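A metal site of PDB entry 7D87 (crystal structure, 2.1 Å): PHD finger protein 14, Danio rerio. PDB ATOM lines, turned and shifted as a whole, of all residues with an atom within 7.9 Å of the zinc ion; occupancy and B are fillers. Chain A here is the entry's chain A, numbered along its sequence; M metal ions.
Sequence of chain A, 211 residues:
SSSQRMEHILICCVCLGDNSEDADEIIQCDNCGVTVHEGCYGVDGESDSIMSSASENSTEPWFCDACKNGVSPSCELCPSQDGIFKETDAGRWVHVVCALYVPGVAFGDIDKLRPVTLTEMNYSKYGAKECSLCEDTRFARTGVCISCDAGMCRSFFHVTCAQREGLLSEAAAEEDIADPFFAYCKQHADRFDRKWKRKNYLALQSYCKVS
The backbone carbonyl oxygen (O) of Asn 19 sits at hydrogen-bond distance from a ring nitrogen (NE2) of His 37 (2.7 Å).
The side-chain sulfur (SG) of Cys 15 sits close to the backbone NH (N) of Gly 17 (3.3 Å).
N of Val 14 sits close to SG of Cys 12 (3.4 Å).
The backbone carbonyl oxygen (O) of Gly 17 lies within hydrogen-bond range of the backbone NH (N) of Cys 12, 3.0 Å away.
Within 4 Å of the zinc ion: Cys 12, Cys 15, His 37 and Cys 40.
The nearest printed residue that does not touch the zinc ion is Val 14 (4.7 Å).
The zinc ion is bound by ND1 of His 37 (2.1 Å).
The zinc ion is bound by SG of Cys 40 (2.2 Å).
SG of Cys 15 binds the zinc ion (2.3 Å).
SG of Cys 12 binds the zinc ion, 2.3 Å away.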
ATOM      1  N   ILE A  11       8.681  16.297  14.942  1.00  0.00           N
ATOM      2  CA  ILE A  11       9.013  17.716  14.970  1.00  0.00           C
ATOM      3  C   ILE A  11       8.068  18.448  14.051  1.00  0.00           C
ATOM      4  O   ILE A  11       7.809  17.999  12.922  1.00  0.00           O
ATOM      5  CB  ILE A  11      10.485  17.928  14.575  1.00  0.00           C
ATOM      6  CG1 ILE A  11      11.379  17.414  15.702  1.00  0.00           C
ATOM      7  CG2 ILE A  11      10.763  19.399  14.263  1.00  0.00           C
ATOM      8  CD1 ILE A  11      12.821  17.377  15.367  1.00  0.00           C
ATOM      9  N   CYS A  12       7.554  19.595  14.508  1.00  0.00           N
ATOM     10  CA  CYS A  12       6.596  20.380  13.732  1.00  0.00           C
ATOM     11  C   CYS A  12       7.328  21.183  12.653  1.00  0.00           C
ATOM     12  O   CYS A  12       8.248  21.940  12.945  1.00  0.00           O
ATOM     13  CB  CYS A  12       5.822  21.318  14.647  1.00  0.00           C
ATOM     14  SG  CYS A  12       4.803  22.490  13.714  1.00  0.00           S
ATOM     15  N   CYS A  13       6.925  21.028  11.390  1.00  0.00           N
ATOM     16  CA  CYS A  13       7.689  21.677  10.324  1.00  0.00           C
ATOM     17  C   CYS A  13       7.371  23.168  10.186  1.00  0.00           C
ATOM     18  O   CYS A  13       7.965  23.830   9.320  1.00  0.00           O
ATOM     19  CB  CYS A  13       7.461  20.965   8.987  1.00  0.00           C
ATOM     20  SG  CYS A  13       5.852  21.297   8.249  1.00  0.00           S
ATOM     21  N   VAL A  14       6.466  23.711  10.986  1.00  0.00           N
ATOM     22  CA  VAL A  14       6.219  25.139  10.989  1.00  0.00           C
ATOM     23  C   VAL A  14       7.049  25.837  12.049  1.00  0.00           C
ATOM     24  O   VAL A  14       7.783  26.781  11.765  1.00  0.00           O
ATOM     25  CB  VAL A  14       4.723  25.428  11.177  1.00  0.00           C
ATOM     26  CG1 VAL A  14       4.500  26.923  11.356  1.00  0.00           C
ATOM     27  CG2 VAL A  14       3.929  24.929   9.968  1.00  0.00           C
ATOM     28  N   CYS A  15       6.959  25.374  13.300  1.00  0.00           N
ATOM     29  CA  CYS A  15       7.620  26.027  14.411  1.00  0.00           C
ATOM     30  C   CYS A  15       8.865  25.297  14.915  1.00  0.00           C
ATOM     31  O   CYS A  15       9.560  25.833  15.781  1.00  0.00           O
ATOM     32  CB  CYS A  15       6.640  26.191  15.588  1.00  0.00           C
ATOM     33  SG  CYS A  15       6.295  24.658  16.529  1.00  0.00           S
ATOM     34  N   LEU A  16       9.144  24.091  14.422  1.00  0.00           N
ATOM     35  CA  LEU A  16      10.284  23.256  14.830  1.00  0.00           C
ATOM     36  C   LEU A  16      10.226  22.868  16.309  1.00  0.00           C
ATOM     37  O   LEU A  16      11.244  22.448  16.864  1.00  0.00           O
ATOM     38  CB  LEU A  16      11.624  23.939  14.538  1.00  0.00           C
ATOM     39  CG  LEU A  16      11.828  24.314  13.079  1.00  0.00           C
ATOM     40  CD1 LEU A  16      13.136  25.077  12.940  1.00  0.00           C
ATOM     41  CD2 LEU A  16      11.817  23.052  12.233  1.00  0.00           C
ATOM     42  N   GLY A  17       9.057  22.996  16.950  1.00  0.00           N
ATOM     43  CA  GLY A  17       8.905  22.473  18.293  1.00  0.00           C
ATOM     44  C   GLY A  17       8.731  20.970  18.294  1.00  0.00           C
ATOM     45  O   GLY A  17       8.376  20.349  17.287  1.00  0.00           O
ATOM     46  N   ASP A  18       8.991  20.353  19.458  1.00  0.00           N
ATOM     47  CA  ASP A  18       8.881  18.908  19.602  1.00  0.00           C
ATOM     48  C   ASP A  18       7.846  18.462  20.625  1.00  0.00           C
ATOM     49  O   ASP A  18       7.721  17.260  20.880  1.00  0.00           O
ATOM     50  CB  ASP A  18      10.243  18.301  19.975  1.00  0.00           C
ATOM     51  CG  ASP A  18      10.878  18.990  21.175  1.00  0.00           C
ATOM     52  OD1 ASP A  18      10.215  19.844  21.808  1.00  0.00           O
ATOM     53  OD2 ASP A  18      12.050  18.670  21.480  1.00  0.00           O
ATOM     54  N   ASN A  19       7.104  19.382  21.232  1.00  0.00           N
ATOM     55  CA  ASN A  19       6.126  18.996  22.229  1.00  0.00           C
ATOM     56  C   ASN A  19       4.846  18.551  21.553  1.00  0.00           C
ATOM     57  O   ASN A  19       4.281  19.268  20.726  1.00  0.00           O
ATOM     58  CB  ASN A  19       5.853  20.144  23.197  1.00  0.00           C
ATOM     59  CG  ASN A  19       6.658  20.033  24.469  1.00  0.00           C
ATOM     60  OD1 ASN A  19       6.493  19.082  25.243  1.00  0.00           O
ATOM     61  ND2 ASN A  19       7.536  21.013  24.693  1.00  0.00           N
ATOM     62  N   ASP A  24      -2.474  19.709  21.771  1.00  0.00           N
ATOM     63  CA  ASP A  24      -1.829  20.133  20.521  1.00  0.00           C
ATOM     64  C   ASP A  24      -0.853  19.039  20.099  1.00  0.00           C
ATOM     65  O   ASP A  24       0.317  19.027  20.500  1.00  0.00           O
ATOM     66  CB  ASP A  24      -1.135  21.481  20.691  1.00  0.00           C
ATOM     67  CG  ASP A  24      -0.824  22.139  19.359  1.00  0.00           C
ATOM     68  OD1 ASP A  24      -1.210  21.568  18.320  1.00  0.00           O
ATOM     69  OD2 ASP A  24      -0.186  23.217  19.351  1.00  0.00           O
ATOM     70  N   GLU A  25      -1.332  18.127  19.272  1.00  0.00           N
ATOM     71  CA  GLU A  25      -0.556  16.974  18.858  1.00  0.00           C
ATOM     72  C   GLU A  25       0.211  17.273  17.582  1.00  0.00           C
ATOM     73  O   GLU A  25      -0.278  18.004  16.707  1.00  0.00           O
ATOM     74  CB  GLU A  25      -1.476  15.769  18.650  1.00  0.00           C
ATOM     75  CG  GLU A  25      -0.785  14.505  18.188  1.00  0.00           C
ATOM     76  CD  GLU A  25      -1.759  13.414  17.767  1.00  0.00           C
ATOM     77  OE1 GLU A  25      -2.970  13.693  17.696  1.00  0.00           O
ATOM     78  OE2 GLU A  25      -1.300  12.282  17.510  1.00  0.00           O
ATOM     79  N   ILE A  26       1.415  16.727  17.481  1.00  0.00           N
ATOM     80  CA  ILE A  26       2.145  16.724  16.215  1.00  0.00           C
ATOM     81  C   ILE A  26       1.644  15.550  15.383  1.00  0.00           C
ATOM     82  O   ILE A  26       1.755  14.394  15.805  1.00  0.00           O
ATOM     83  CB  ILE A  26       3.650  16.633  16.448  1.00  0.00           C
ATOM     84  CG1 ILE A  26       4.159  17.877  17.177  1.00  0.00           C
ATOM     85  CG2 ILE A  26       4.381  16.456  15.130  1.00  0.00           C
ATOM     86  CD1 ILE A  26       5.626  17.805  17.609  1.00  0.00           C
ATOM     87  N   THR A  35       5.045  16.607   8.950  1.00  0.00           N
ATOM     88  CA  THR A  35       4.605  16.547  10.337  1.00  0.00           C
ATOM     89  C   THR A  35       4.416  17.962  10.867  1.00  0.00           C
ATOM     90  O   THR A  35       5.239  18.839  10.593  1.00  0.00           O
ATOM     91  CB  THR A  35       5.625  15.788  11.197  1.00  0.00           C
ATOM     92  OG1 THR A  35       6.930  16.334  10.958  1.00  0.00           O
ATOM     93  CG2 THR A  35       5.661  14.300  10.834  1.00  0.00           C
ATOM     94  N   VAL A  36       3.334  18.201  11.616  1.00  0.00           N
ATOM     95  CA  VAL A  36       2.957  19.554  12.034  1.00  0.00           C
ATOM     96  C   VAL A  36       2.112  19.480  13.301  1.00  0.00           C
ATOM     97  O   VAL A  36       1.367  18.522  13.510  1.00  0.00           O
ATOM     98  CB  VAL A  36       2.206  20.281  10.882  1.00  0.00           C
ATOM     99  CG1 VAL A  36       0.856  19.614  10.592  1.00  0.00           C
ATOM    100  CG2 VAL A  36       2.023  21.778  11.202  1.00  0.00           C
ATOM    101  N   HIS A  37       2.248  20.501  14.150  1.00  0.00           N
ATOM    102  CA  HIS A  37       1.272  20.695  15.223  1.00  0.00           C
ATOM    103  C   HIS A  37      -0.117  20.921  14.623  1.00  0.00           C
ATOM    104  O   HIS A  37      -0.270  21.649  13.638  1.00  0.00           O
ATOM    105  CB  HIS A  37       1.628  21.913  16.094  1.00  0.00           C
ATOM    106  CG  HIS A  37       2.748  21.682  17.057  1.00  0.00           C
ATOM    107  ND1 HIS A  37       3.894  22.446  17.055  1.00  0.00           N
ATOM    108  CD2 HIS A  37       2.871  20.817  18.088  1.00  0.00           C
ATOM    109  CE1 HIS A  37       4.694  22.037  18.027  1.00  0.00           C
ATOM    110  NE2 HIS A  37       4.098  21.052  18.668  1.00  0.00           N
ATOM    111  N   GLU A  38      -1.121  20.313  15.248  1.00  0.00           N
ATOM    112  CA  GLU A  38      -2.510  20.660  14.925  1.00  0.00           C
ATOM    113  C   GLU A  38      -2.721  22.158  15.006  1.00  0.00           C
ATOM    114  O   GLU A  38      -3.282  22.780  14.102  1.00  0.00           O
ATOM    115  CB  GLU A  38      -3.460  19.946  15.891  1.00  0.00           C
ATOM    116  CG  GLU A  38      -3.321  18.443  15.920  1.00  0.00           C
ATOM    117  CD  GLU A  38      -4.142  17.817  17.033  1.00  0.00           C
ATOM    118  OE1 GLU A  38      -3.913  18.169  18.217  1.00  0.00           O
ATOM    119  OE2 GLU A  38      -5.018  16.994  16.722  1.00  0.00           O
ATOM    120  N   GLY A  39      -2.245  22.773  16.098  1.00  0.00           N
ATOM    121  CA  GLY A  39      -2.421  24.197  16.331  1.00  0.00           C
ATOM    122  C   GLY A  39      -1.631  25.074  15.379  1.00  0.00           C
ATOM    123  O   GLY A  39      -2.013  26.215  15.155  1.00  0.00           O
ATOM    124  N   CYS A  40      -0.536  24.556  14.823  1.00  0.00           N
ATOM    125  CA  CYS A  40       0.205  25.348  13.844  1.00  0.00           C
ATOM    126  C   CYS A  40      -0.401  25.269  12.454  1.00  0.00           C
ATOM    127  O   CYS A  40       0.049  25.988  11.557  1.00  0.00           O
ATOM    128  CB  CYS A  40       1.679  24.910  13.799  1.00  0.00           C
ATOM    129  SG  CYS A  40       2.685  25.233  15.308  1.00  0.00           S
ATOM    130  N   TYR A  41      -1.426  24.448  12.240  1.00  0.00           N
ATOM    131  CA  TYR A  41      -2.005  24.249  10.919  1.00  0.00           C
ATOM    132  C   TYR A  41      -3.505  24.452  10.885  1.00  0.00           C
ATOM    133  O   TYR A  41      -4.108  24.321   9.816  1.00  0.00           O
ATOM    134  CB  TYR A  41      -1.682  22.837  10.400  1.00  0.00           C
ATOM    135  CG  TYR A  41      -1.849  22.607   8.908  1.00  0.00           C
ATOM    136  CD1 TYR A  41      -1.028  23.241   7.983  1.00  0.00           C
ATOM    137  CD2 TYR A  41      -2.802  21.715   8.424  1.00  0.00           C
ATOM    138  CE1 TYR A  41      -1.162  23.008   6.618  1.00  0.00           C
ATOM    139  CE2 TYR A  41      -2.942  21.482   7.067  1.00  0.00           C
ATOM    140  CZ  TYR A  41      -2.116  22.131   6.168  1.00  0.00           C
ATOM    141  OH  TYR A  41      -2.248  21.894   4.816  1.00  0.00           O
ATOM    142  N   GLU A 170       9.502  32.985  17.649  1.00  0.00           N
ATOM    143  CA  GLU A 170       8.144  33.356  17.944  1.00  0.00           C
ATOM    144  C   GLU A 170       8.099  33.801  19.391  1.00  0.00           C
ATOM    145  O   GLU A 170       8.555  33.059  20.270  1.00  0.00           O
ATOM    146  CB  GLU A 170       7.194  32.192  17.693  1.00  0.00           C
ATOM    147  CG  GLU A 170       5.719  32.501  17.964  1.00  0.00           C
ATOM    148  CD  GLU A 170       4.830  31.282  17.717  1.00  0.00           C
ATOM    149  OE1 GLU A 170       3.614  31.354  18.002  1.00  0.00           O
ATOM    150  OE2 GLU A 170       5.356  30.242  17.240  1.00  0.00           O
HETATM  151 ZN    ZN M   1       4.412  23.829  15.544  1.00  0.00          ZN
